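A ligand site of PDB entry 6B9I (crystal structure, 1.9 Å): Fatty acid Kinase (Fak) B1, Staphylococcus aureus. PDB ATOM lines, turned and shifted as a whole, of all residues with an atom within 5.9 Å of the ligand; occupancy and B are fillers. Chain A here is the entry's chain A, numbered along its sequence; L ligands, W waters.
The side-chain hydroxyl (OG) of Ser 95 sits at hydrogen-bond distance from an oxygen (O2) of the ligand (2.5 Å). OG1 of Thr 62 sits at hydrogen-bond distance from O1 of the ligand, at 2.7 Å.
Water W3 lies within hydrogen-bond range of an oxygen (O2) of the ligand (2.8 Å), the backbone NH of Gly 96 (2.9 Å) and the side-chain amide oxygen of Gln 64 (3.1 Å). Water W2 bridges the backbone NH of Gln 64 (2.8 Å) and an oxygen (O1) of the ligand (3.0 Å). Water W1 lies within hydrogen-bond range of O1 of the ligand (3.3 Å) and O of Thr 62 (3.5 Å).
Merely in contact with the ligand: Leu 28 (3.7 Å), Ser 63 (3.5 Å), Gln 64 (3.6 Å), Ile 94 (3.4 Å), Leu 120 (3.9 Å), Ala 121 (3.7 Å), Ile 124 (3.97 Å), Ala 158 (3.7 Å), Tyr 159 (3.7 Å), Leu 160 (3.7 Å), Arg 173 (3.9 Å), Phe 193 (3.7 Å), Ile 198 (3.9 Å), Ile 233 (3.7 Å), Phe 263 (3.7 Å), Val 266 (3.9 Å), Val 267 (3.9 Å), His 270 (3.6 Å), Leu 271 (3.7 Å), Gly 277 (3.8 Å), Leu 278 (3.8 Å) and Gly 279 (3.4 Å). Hydrophobic or aromatic side chains that line the ligand: Leu 28, Ile 94, Leu 120, Ala 121, Ile 124, Ala 158, Leu 160, Phe 193, Ile 198, Ile 233, Phe 263, Val 266, Val 267, His 270 and Leu 271. Within 4 Å of the ligand: Leu 28, Thr 62, Ser 63, Gln 64, Ile 94, Ser 95, Leu 120, Ala 121, Ile 124, Ala 158, Tyr 159, Leu 160, Arg 173, Phe 193, Ile 198, Ile 233, Phe 263, Val 266, Val 267, His 270, Leu 271, Gly 277, Leu 278 and Gly 279.
The side-chain hydroxyl (OG) of Ser 95 is in hydrogen-bond range of the backbone NH (N) of Ser 97, 3.1 Å away. The backbone NH (N) of Leu 278 sits at hydrogen-bond distance from the backbone carbonyl oxygen (O) of Tyr 159. The backbone carbonyl oxygen of Ser 29 lies within hydrogen-bond range of the backbone NH of Ser 63. The backbone carbonyl oxygen (O) of Gly 96 is in hydrogen-bond range of the side-chain amide nitrogen (NE2) of Gln 64 (3.5 Å). The backbone carbonyl oxygen of Ala 158 lies within hydrogen-bond range of the backbone NH of Phe 193, at 3.0 Å. The guanidinium group of Arg 173 lies within hydrogen-bond range of the backbone carbonyl oxygen of Ile 94 (2.8 Å). The backbone carbonyl oxygen (O) of Leu 168 sits at hydrogen-bond distance from the backbone NH (N) of Arg 173 (3.0 Å). The backbone NH (N) of Leu 168 is in hydrogen-bond range of the backbone carbonyl oxygen (O) of His 270 (3.0 Å).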
ATOM      1  N   THR A  10     -17.667  -9.643  16.810  1.00  0.00           N
ATOM      2  CA  THR A  10     -18.528 -10.456  17.657  1.00  0.00           C
ATOM      3  C   THR A  10     -19.770 -10.971  16.940  1.00  0.00           C
ATOM      4  O   THR A  10     -20.590 -11.651  17.576  1.00  0.00           O
ATOM      5  CB  THR A  10     -18.964  -9.666  18.899  1.00  0.00           C
ATOM      6  OG1 THR A  10     -19.253  -8.312  18.538  1.00  0.00           O
ATOM      7  CG2 THR A  10     -17.864  -9.700  19.954  1.00  0.00           C
ATOM      8  N   LEU A  28     -12.690  -6.828  17.721  1.00  0.00           N
ATOM      9  CA  LEU A  28     -12.480  -6.640  19.147  1.00  0.00           C
ATOM     10  C   LEU A  28     -11.268  -7.465  19.587  1.00  0.00           C
ATOM     11  O   LEU A  28     -10.756  -8.315  18.849  1.00  0.00           O
ATOM     12  CB  LEU A  28     -13.731  -7.026  19.937  1.00  0.00           C
ATOM     13  CG  LEU A  28     -14.921  -6.064  19.791  1.00  0.00           C
ATOM     14  CD1 LEU A  28     -15.778  -6.379  18.548  1.00  0.00           C
ATOM     15  CD2 LEU A  28     -15.785  -6.091  21.044  1.00  0.00           C
ATOM     16  N   SER A  29     -10.791  -7.211  20.808  1.00  0.00           N
ATOM     17  CA  SER A  29      -9.578  -7.846  21.293  1.00  0.00           C
ATOM     18  C   SER A  29      -9.766  -8.381  22.702  1.00  0.00           C
ATOM     19  O   SER A  29     -10.682  -7.971  23.426  1.00  0.00           O
ATOM     20  CB  SER A  29      -8.392  -6.873  21.253  1.00  0.00           C
ATOM     21  OG  SER A  29      -8.539  -5.844  22.222  1.00  0.00           O
ATOM     22  N   THR A  62     -11.549  -7.516  27.765  1.00  0.00           N
ATOM     23  CA  THR A  62     -11.797  -7.322  26.350  1.00  0.00           C
ATOM     24  C   THR A  62     -11.842  -5.833  26.015  1.00  0.00           C
ATOM     25  O   THR A  62     -12.001  -4.984  26.897  1.00  0.00           O
ATOM     26  CB  THR A  62     -13.111  -7.979  25.925  1.00  0.00           C
ATOM     27  OG1 THR A  62     -14.206  -7.371  26.619  1.00  0.00           O
ATOM     28  CG2 THR A  62     -13.082  -9.470  26.247  1.00  0.00           C
ATOM     29  N   SER A  63     -11.692  -5.531  24.727  1.00  0.00           N
ATOM     30  CA  SER A  63     -11.729  -4.171  24.231  1.00  0.00           C
ATOM     31  C   SER A  63     -12.628  -4.109  23.005  1.00  0.00           C
ATOM     32  O   SER A  63     -12.543  -4.964  22.124  1.00  0.00           O
ATOM     33  CB  SER A  63     -10.332  -3.654  23.875  1.00  0.00           C
ATOM     34  OG  SER A  63      -9.437  -3.786  24.963  1.00  0.00           O
ATOM     35  N   GLN A  64     -13.496  -3.105  22.970  1.00  0.00           N
ATOM     36  CA  GLN A  64     -14.252  -2.772  21.781  1.00  0.00           C
ATOM     37  C   GLN A  64     -13.284  -2.315  20.695  1.00  0.00           C
ATOM     38  O   GLN A  64     -12.125  -2.013  20.975  1.00  0.00           O
ATOM     39  CB  GLN A  64     -15.251  -1.665  22.108  1.00  0.00           C
ATOM     40  CG  GLN A  64     -14.550  -0.355  22.484  1.00  0.00           C
ATOM     41  CD  GLN A  64     -15.495   0.810  22.561  1.00  0.00           C
ATOM     42  OE1 GLN A  64     -16.237   0.966  23.529  1.00  0.00           O
ATOM     43  NE2 GLN A  64     -15.482   1.654  21.535  1.00  0.00           N
ATOM     44  N   LEU A  90     -22.452  -5.119  17.821  1.00  0.00           N
ATOM     45  CA  LEU A  90     -22.727  -5.715  19.120  1.00  0.00           C
ATOM     46  C   LEU A  90     -23.678  -4.843  19.922  1.00  0.00           C
ATOM     47  O   LEU A  90     -23.722  -3.617  19.746  1.00  0.00           O
ATOM     48  CB  LEU A  90     -21.406  -5.903  19.870  1.00  0.00           C
ATOM     49  CG  LEU A  90     -21.304  -6.659  21.189  1.00  0.00           C
ATOM     50  CD1 LEU A  90     -21.710  -8.104  21.016  1.00  0.00           C
ATOM     51  CD2 LEU A  90     -19.863  -6.583  21.692  1.00  0.00           C
ATOM     52  N   ILE A  94     -24.028  -3.952  26.252  1.00  0.00           N
ATOM     53  CA  ILE A  94     -22.908  -4.694  26.807  1.00  0.00           C
ATOM     54  C   ILE A  94     -21.556  -4.203  26.290  1.00  0.00           C
ATOM     55  O   ILE A  94     -20.521  -4.706  26.741  1.00  0.00           O
ATOM     56  CB  ILE A  94     -23.052  -6.206  26.535  1.00  0.00           C
ATOM     57  CG1 ILE A  94     -22.940  -6.498  25.037  1.00  0.00           C
ATOM     58  CG2 ILE A  94     -24.375  -6.714  27.081  1.00  0.00           C
ATOM     59  CD1 ILE A  94     -23.213  -7.943  24.672  1.00  0.00           C
ATOM     60  N   SER A  95     -21.543  -3.234  25.379  1.00  0.00           N
ATOM     61  CA  SER A  95     -20.286  -2.785  24.798  1.00  0.00           C
ATOM     62  C   SER A  95     -20.486  -1.396  24.213  1.00  0.00           C
ATOM     63  O   SER A  95     -21.592  -1.022  23.822  1.00  0.00           O
ATOM     64  CB  SER A  95     -19.798  -3.749  23.711  1.00  0.00           C
ATOM     65  OG  SER A  95     -18.625  -3.284  23.070  1.00  0.00           O
ATOM     66  N   GLY A  96     -19.399  -0.632  24.165  1.00  0.00           N
ATOM     67  CA  GLY A  96     -19.395   0.652  23.502  1.00  0.00           C
ATOM     68  C   GLY A  96     -19.095   0.576  22.023  1.00  0.00           C
ATOM     69  O   GLY A  96     -18.937   1.625  21.383  1.00  0.00           O
ATOM     70  N   SER A  97     -19.008  -0.625  21.460  1.00  0.00           N
ATOM     71  CA  SER A  97     -18.669  -0.762  20.045  1.00  0.00           C
ATOM     72  C   SER A  97     -19.677  -0.043  19.156  1.00  0.00           C
ATOM     73  O   SER A  97     -19.302   0.574  18.150  1.00  0.00           O
ATOM     74  CB  SER A  97     -18.583  -2.245  19.665  1.00  0.00           C
ATOM     75  OG  SER A  97     -18.517  -2.410  18.259  1.00  0.00           O
ATOM     76  N   LEU A 120     -27.934  -7.520  20.381  1.00  0.00           N
ATOM     77  CA  LEU A 120     -27.579  -8.880  20.771  1.00  0.00           C
ATOM     78  C   LEU A 120     -26.116  -9.147  20.431  1.00  0.00           C
ATOM     79  O   LEU A 120     -25.290  -8.228  20.496  1.00  0.00           O
ATOM     80  CB  LEU A 120     -28.503  -9.892  20.106  1.00  0.00           C
ATOM     81  CG  LEU A 120     -29.123 -10.823  21.160  1.00  0.00           C
ATOM     82  CD1 LEU A 120     -30.507 -11.311  20.766  1.00  0.00           C
ATOM     83  CD2 LEU A 120     -28.206 -11.996  21.478  1.00  0.00           C
ATOM     84  N   ALA A 121     -25.783 -10.386  20.085  1.00  0.00           N
ATOM     85  CA  ALA A 121     -24.384 -10.800  19.974  1.00  0.00           C
ATOM     86  C   ALA A 121     -24.307 -12.120  19.219  1.00  0.00           C
ATOM     87  O   ALA A 121     -25.308 -12.809  19.022  1.00  0.00           O
ATOM     88  CB  ALA A 121     -23.743 -10.945  21.360  1.00  0.00           C
ATOM     89  N   ALA A 122     -23.085 -12.469  18.819  1.00  0.00           N
ATOM     90  CA  ALA A 122     -22.772 -13.748  18.157  1.00  0.00           C
ATOM     91  C   ALA A 122     -23.571 -13.828  16.851  1.00  0.00           C
ATOM     92  O   ALA A 122     -23.911 -12.802  16.244  1.00  0.00           O
ATOM     93  CB  ALA A 122     -22.992 -14.898  19.121  1.00  0.00           C
ATOM     94  N   ILE A 124     -26.574 -14.383  16.191  1.00  0.00           N
ATOM     95  CA  ILE A 124     -27.820 -13.631  16.135  1.00  0.00           C
ATOM     96  C   ILE A 124     -27.558 -12.219  15.639  1.00  0.00           C
ATOM     97  O   ILE A 124     -28.289 -11.687  14.796  1.00  0.00           O
ATOM     98  CB  ILE A 124     -28.528 -13.649  17.497  1.00  0.00           C
ATOM     99  CG1 ILE A 124     -28.867 -15.082  17.914  1.00  0.00           C
ATOM    100  CG2 ILE A 124     -29.797 -12.814  17.439  1.00  0.00           C
ATOM    101  CD1 ILE A 124     -29.842 -15.797  16.977  1.00  0.00           C
ATOM    102  N   GLY A 157     -34.463 -12.666  19.757  1.00  0.00           N
ATOM    103  CA  GLY A 157     -34.106 -12.745  21.167  1.00  0.00           C
ATOM    104  C   GLY A 157     -33.205 -13.926  21.421  1.00  0.00           C
ATOM    105  O   GLY A 157     -32.780 -14.629  20.496  1.00  0.00           O
ATOM    106  N   ALA A 158     -32.899 -14.142  22.705  1.00  0.00           N
ATOM    107  CA  ALA A 158     -31.978 -15.202  23.082  1.00  0.00           C
ATOM    108  C   ALA A 158     -32.067 -15.472  24.576  1.00  0.00           C
ATOM    109  O   ALA A 158     -32.288 -14.565  25.377  1.00  0.00           O
ATOM    110  CB  ALA A 158     -30.529 -14.824  22.716  1.00  0.00           C
ATOM    111  N   TYR A 159     -31.890 -16.751  24.924  1.00  0.00           N
ATOM    112  CA  TYR A 159     -31.724 -17.220  26.285  1.00  0.00           C
ATOM    113  C   TYR A 159     -30.387 -17.924  26.394  1.00  0.00           C
ATOM    114  O   TYR A 159     -29.831 -18.376  25.385  1.00  0.00           O
ATOM    115  CB  TYR A 159     -32.870 -18.176  26.689  1.00  0.00           C
ATOM    116  CG  TYR A 159     -34.220 -17.493  26.814  1.00  0.00           C
ATOM    117  CD1 TYR A 159     -34.941 -17.116  25.690  1.00  0.00           C
ATOM    118  CD2 TYR A 159     -34.778 -17.240  28.062  1.00  0.00           C
ATOM    119  CE1 TYR A 159     -36.171 -16.497  25.798  1.00  0.00           C
ATOM    120  CE2 TYR A 159     -36.015 -16.634  28.182  1.00  0.00           C
ATOM    121  CZ  TYR A 159     -36.704 -16.255  27.047  1.00  0.00           C
ATOM    122  OH  TYR A 159     -37.933 -15.650  27.156  1.00  0.00           O
ATOM    123  N   LEU A 160     -29.845 -18.028  27.614  1.00  0.00           N
ATOM    124  CA  LEU A 160     -28.528 -18.625  27.748  1.00  0.00           C
ATOM    125  C   LEU A 160     -28.245 -19.057  29.180  1.00  0.00           C
ATOM    126  O   LEU A 160     -28.919 -18.628  30.116  1.00  0.00           O
ATOM    127  CB  LEU A 160     -27.424 -17.664  27.280  1.00  0.00           C
ATOM    128  CG  LEU A 160     -27.155 -16.504  28.241  1.00  0.00           C
ATOM    129  CD1 LEU A 160     -25.662 -16.164  28.260  1.00  0.00           C
ATOM    130  CD2 LEU A 160     -27.982 -15.296  27.838  1.00  0.00           C
ATOM    131  N   LEU A 168     -19.293 -12.930  34.201  1.00  0.00           N
ATOM    132  CA  LEU A 168     -20.255 -11.866  33.900  1.00  0.00           C
ATOM    133  C   LEU A 168     -20.298 -10.836  35.019  1.00  0.00           C
ATOM    134  O   LEU A 168     -20.418  -9.631  34.747  1.00  0.00           O
ATOM    135  CB  LEU A 168     -21.648 -12.473  33.685  1.00  0.00           C
ATOM    136  CG  LEU A 168     -21.907 -13.184  32.351  1.00  0.00           C
ATOM    137  CD1 LEU A 168     -23.256 -13.891  32.395  1.00  0.00           C
ATOM    138  CD2 LEU A 168     -21.845 -12.200  31.189  1.00  0.00           C
ATOM    139  N   ARG A 173     -21.491  -7.385  33.121  1.00  0.00           N
ATOM    140  CA  ARG A 173     -22.352  -7.647  31.977  1.00  0.00           C
ATOM    141  C   ARG A 173     -23.582  -8.472  32.334  1.00  0.00           C
ATOM    142  O   ARG A 173     -24.359  -8.832  31.443  1.00  0.00           O
ATOM    143  CB  ARG A 173     -21.566  -8.333  30.863  1.00  0.00           C
ATOM    144  CG  ARG A 173     -21.067  -7.364  29.782  1.00  0.00           C
ATOM    145  CD  ARG A 173     -20.027  -6.382  30.339  1.00  0.00           C
ATOM    146  NE  ARG A 173     -19.527  -5.488  29.289  1.00  0.00           N
ATOM    147  CZ  ARG A 173     -18.437  -4.737  29.398  1.00  0.00           C
ATOM    148  NH1 ARG A 173     -17.714  -4.765  30.517  1.00  0.00           N
ATOM    149  NH2 ARG A 173     -18.062  -3.956  28.394  1.00  0.00           N
ATOM    150  N   PHE A 193     -31.686 -12.148  27.062  1.00  0.00           N
ATOM    151  CA  PHE A 193     -31.473 -10.787  26.595  1.00  0.00           C
ATOM    152  C   PHE A 193     -32.781 -10.007  26.658  1.00  0.00           C
ATOM    153  O   PHE A 193     -33.844 -10.511  26.281  1.00  0.00           O
ATOM    154  CB  PHE A 193     -30.933 -10.782  25.159  1.00  0.00           C
ATOM    155  CG  PHE A 193     -29.432 -10.714  25.083  1.00  0.00           C
ATOM    156  CD1 PHE A 193     -28.658 -11.855  25.265  1.00  0.00           C
ATOM    157  CD2 PHE A 193     -28.794  -9.513  24.832  1.00  0.00           C
ATOM    158  CE1 PHE A 193     -27.283 -11.789  25.196  1.00  0.00           C
ATOM    159  CE2 PHE A 193     -27.413  -9.432  24.767  1.00  0.00           C
ATOM    160  CZ  PHE A 193     -26.664 -10.574  24.949  1.00  0.00           C
ATOM    161  N   ILE A 198     -28.318  -8.358  29.580  1.00  0.00           N
ATOM    162  CA  ILE A 198     -28.433  -9.725  30.066  1.00  0.00           C
ATOM    163  C   ILE A 198     -28.976  -9.689  31.479  1.00  0.00           C
ATOM    164  O   ILE A 198     -28.357  -9.099  32.372  1.00  0.00           O
ATOM    165  CB  ILE A 198     -27.082 -10.465  30.004  1.00  0.00           C
ATOM    166  CG1 ILE A 198     -26.533 -10.459  28.574  1.00  0.00           C
ATOM    167  CG2 ILE A 198     -27.224 -11.887  30.524  1.00  0.00           C
ATOM    168  CD1 ILE A 198     -25.137 -11.009  28.459  1.00  0.00           C
ATOM    169  N   PHE A 231     -30.733 -20.500  16.434  1.00  0.00           N
ATOM    170  CA  PHE A 231     -29.299 -20.720  16.531  1.00  0.00           C
ATOM    171  C   PHE A 231     -28.977 -21.291  17.901  1.00  0.00           C
ATOM    172  O   PHE A 231     -29.228 -20.643  18.925  1.00  0.00           O
ATOM    173  CB  PHE A 231     -28.517 -19.426  16.317  1.00  0.00           C
ATOM    174  CG  PHE A 231     -27.944 -19.299  14.934  1.00  0.00           C
ATOM    175  CD1 PHE A 231     -26.719 -19.882  14.614  1.00  0.00           C
ATOM    176  CD2 PHE A 231     -28.628 -18.599  13.953  1.00  0.00           C
ATOM    177  CE1 PHE A 231     -26.194 -19.764  13.336  1.00  0.00           C
ATOM    178  CE2 PHE A 231     -28.102 -18.481  12.675  1.00  0.00           C
ATOM    179  CZ  PHE A 231     -26.885 -19.063  12.367  1.00  0.00           C
ATOM    180  N   ILE A 233     -25.873 -21.777  20.030  1.00  0.00           N
ATOM    181  CA  ILE A 233     -24.533 -21.199  20.062  1.00  0.00           C
ATOM    182  C   ILE A 233     -23.826 -21.745  21.295  1.00  0.00           C
ATOM    183  O   ILE A 233     -24.183 -21.408  22.430  1.00  0.00           O
ATOM    184  CB  ILE A 233     -24.557 -19.669  20.061  1.00  0.00           C
ATOM    185  CG1 ILE A 233     -25.490 -19.157  18.948  1.00  0.00           C
ATOM    186  CG2 ILE A 233     -23.160 -19.121  19.875  1.00  0.00           C
ATOM    187  CD1 ILE A 233     -25.262 -17.709  18.564  1.00  0.00           C
ATOM    188  N   PHE A 263     -19.260 -19.442  20.396  1.00  0.00           N
ATOM    189  CA  PHE A 263     -18.785 -18.154  20.891  1.00  0.00           C
ATOM    190  C   PHE A 263     -17.289 -17.998  20.626  1.00  0.00           C
ATOM    191  O   PHE A 263     -16.502 -18.928  20.834  1.00  0.00           O
ATOM    192  CB  PHE A 263     -19.041 -18.015  22.398  1.00  0.00           C
ATOM    193  CG  PHE A 263     -20.487 -18.106  22.789  1.00  0.00           C
ATOM    194  CD1 PHE A 263     -21.391 -17.125  22.385  1.00  0.00           C
ATOM    195  CD2 PHE A 263     -20.942 -19.158  23.559  1.00  0.00           C
ATOM    196  CE1 PHE A 263     -22.728 -17.201  22.757  1.00  0.00           C
ATOM    197  CE2 PHE A 263     -22.274 -19.241  23.926  1.00  0.00           C
ATOM    198  CZ  PHE A 263     -23.165 -18.267  23.522  1.00  0.00           C
ATOM    199  N   VAL A 266     -13.911 -13.044  22.638  1.00  0.00           N
ATOM    200  CA  VAL A 266     -14.384 -11.851  23.355  1.00  0.00           C
ATOM    201  C   VAL A 266     -15.628 -12.170  24.173  1.00  0.00           C
ATOM    202  O   VAL A 266     -15.723 -11.822  25.352  1.00  0.00           O
ATOM    203  CB  VAL A 266     -14.623 -10.695  22.380  1.00  0.00           C
ATOM    204  CG1 VAL A 266     -15.466  -9.609  23.033  1.00  0.00           C
ATOM    205  CG2 VAL A 266     -13.297 -10.122  21.920  1.00  0.00           C
ATOM    206  N   VAL A 267     -16.601 -12.853  23.564  1.00  0.00           N
ATOM    207  CA  VAL A 267     -17.800 -13.234  24.295  1.00  0.00           C
ATOM    208  C   VAL A 267     -17.476 -14.307  25.325  1.00  0.00           C
ATOM    209  O   VAL A 267     -17.990 -14.282  26.450  1.00  0.00           O
ATOM    210  CB  VAL A 267     -18.908 -13.669  23.332  1.00  0.00           C
ATOM    211  CG1 VAL A 267     -20.019 -14.390  24.078  1.00  0.00           C
ATOM    212  CG2 VAL A 267     -19.468 -12.458  22.597  1.00  0.00           C
ATOM    213  N   HIS A 270     -16.392 -13.205  28.799  1.00  0.00           N
ATOM    214  CA  HIS A 270     -17.411 -12.712  29.724  1.00  0.00           C
ATOM    215  C   HIS A 270     -18.316 -13.810  30.234  1.00  0.00           C
ATOM    216  O   HIS A 270     -18.839 -13.708  31.357  1.00  0.00           O
ATOM    217  CB  HIS A 270     -18.249 -11.616  29.060  1.00  0.00           C
ATOM    218  CG  HIS A 270     -17.468 -10.366  28.751  1.00  0.00           C
ATOM    219  ND1 HIS A 270     -17.556  -9.230  29.524  1.00  0.00           N
ATOM    220  CD2 HIS A 270     -16.588 -10.085  27.758  1.00  0.00           C
ATOM    221  CE1 HIS A 270     -16.770  -8.297  29.026  1.00  0.00           C
ATOM    222  NE2 HIS A 270     -16.166  -8.786  27.957  1.00  0.00           N
ATOM    223  N   LEU A 271     -18.538 -14.857  29.448  1.00  0.00           N
ATOM    224  CA  LEU A 271     -19.399 -15.951  29.892  1.00  0.00           C
ATOM    225  C   LEU A 271     -18.663 -16.909  30.817  1.00  0.00           C
ATOM    226  O   LEU A 271     -19.277 -17.476  31.732  1.00  0.00           O
ATOM    227  CB  LEU A 271     -19.941 -16.735  28.699  1.00  0.00           C
ATOM    228  CG  LEU A 271     -20.794 -15.966  27.683  1.00  0.00           C
ATOM    229  CD1 LEU A 271     -21.257 -16.919  26.587  1.00  0.00           C
ATOM    230  CD2 LEU A 271     -21.976 -15.309  28.367  1.00  0.00           C
ATOM    231  N   LEU A 276     -23.842 -21.514  26.928  1.00  0.00           N
ATOM    232  CA  LEU A 276     -24.711 -22.125  25.940  1.00  0.00           C
ATOM    233  C   LEU A 276     -25.864 -21.179  25.674  1.00  0.00           C
ATOM    234  O   LEU A 276     -26.563 -20.788  26.619  1.00  0.00           O
ATOM    235  CB  LEU A 276     -25.223 -23.489  26.398  1.00  0.00           C
ATOM    236  CG  LEU A 276     -26.231 -24.190  25.489  1.00  0.00           C
ATOM    237  CD1 LEU A 276     -25.645 -24.399  24.086  1.00  0.00           C
ATOM    238  CD2 LEU A 276     -26.704 -25.509  26.093  1.00  0.00           C
ATOM    239  N   GLY A 277     -26.066 -20.809  24.421  1.00  0.00           N
ATOM    240  CA  GLY A 277     -27.140 -19.903  24.048  1.00  0.00           C
ATOM    241  C   GLY A 277     -28.103 -20.563  23.083  1.00  0.00           C
ATOM    242  O   GLY A 277     -27.721 -21.428  22.289  1.00  0.00           O
ATOM    243  N   LEU A 278     -29.367 -20.149  23.158  1.00  0.00           N
ATOM    244  CA  LEU A 278     -30.386 -20.501  22.175  1.00  0.00           C
ATOM    245  C   LEU A 278     -31.040 -19.212  21.735  1.00  0.00           C
ATOM    246  O   LEU A 278     -31.748 -18.573  22.517  1.00  0.00           O
ATOM    247  CB  LEU A 278     -31.410 -21.482  22.743  1.00  0.00           C
ATOM    248  CG  LEU A 278     -32.518 -21.903  21.778  1.00  0.00           C
ATOM    249  CD1 LEU A 278     -31.933 -22.355  20.445  1.00  0.00           C
ATOM    250  CD2 LEU A 278     -33.379 -23.017  22.387  1.00  0.00           C
ATOM    251  N   GLY A 279     -30.794 -18.807  20.483  1.00  0.00           N
ATOM    252  CA  GLY A 279     -31.318 -17.564  19.971  1.00  0.00           C
ATOM    253  C   GLY A 279     -32.309 -17.785  18.848  1.00  0.00           C
ATOM    254  O   GLY A 279     -32.291 -18.842  18.213  1.00  0.00           O
HETATM  255  C1  LIG L   1     -17.968  -6.643  25.548  1.00  0.00           C
HETATM  256  C2  LIG L   1     -18.479  -8.067  25.310  1.00  0.00           C
HETATM  257  C3  LIG L   1     -19.618  -8.398  26.280  1.00  0.00           C
HETATM  258  C4  LIG L   1     -20.099  -9.840  26.054  1.00  0.00           C
HETATM  259  C5  LIG L   1     -21.115 -10.251  27.130  1.00  0.00           C
HETATM  260  C6  LIG L   1     -21.601 -11.685  26.910  1.00  0.00           C
HETATM  261  C7  LIG L   1     -22.517 -11.774  25.687  1.00  0.00           C
HETATM  262  C8  LIG L   1     -23.295 -13.100  25.654  1.00  0.00           C
HETATM  263  C9  LIG L   1     -23.983 -13.248  24.291  1.00  0.00           C
HETATM  264  C10 LIG L   1     -24.843 -14.519  24.225  1.00  0.00           C
HETATM  265  C11 LIG L   1     -25.593 -14.549  22.891  1.00  0.00           C
HETATM  266  C12 LIG L   1     -26.331 -15.886  22.697  1.00  0.00           C
HETATM  267  C13 LIG L   1     -27.143 -15.846  21.403  1.00  0.00           C
HETATM  268  C14 LIG L   1     -27.265 -16.131  23.884  1.00  0.00           C
HETATM  269  C15 LIG L   1     -27.828 -17.190  21.169  1.00  0.00           C
HETATM  270  C16 LIG L   1     -16.876  -6.298  24.536  1.00  0.00           C
HETATM  271  C17 LIG L   1     -16.175  -4.989  24.913  1.00  0.00           C
HETATM  272  O1  LIG L   1     -15.089  -5.005  25.560  1.00  0.00           O
HETATM  273  O2  LIG L   1     -16.677  -3.883  24.594  1.00  0.00           O
HETATM  274  O   HOH W   1     -14.637  -3.024  28.100  1.00  0.00           O
HETATM  275  O   HOH W   2     -14.132  -2.193  25.501  1.00  0.00           O
HETATM  276  O   HOH W   3     -16.877  -1.275  25.504  1.00  0.00           O
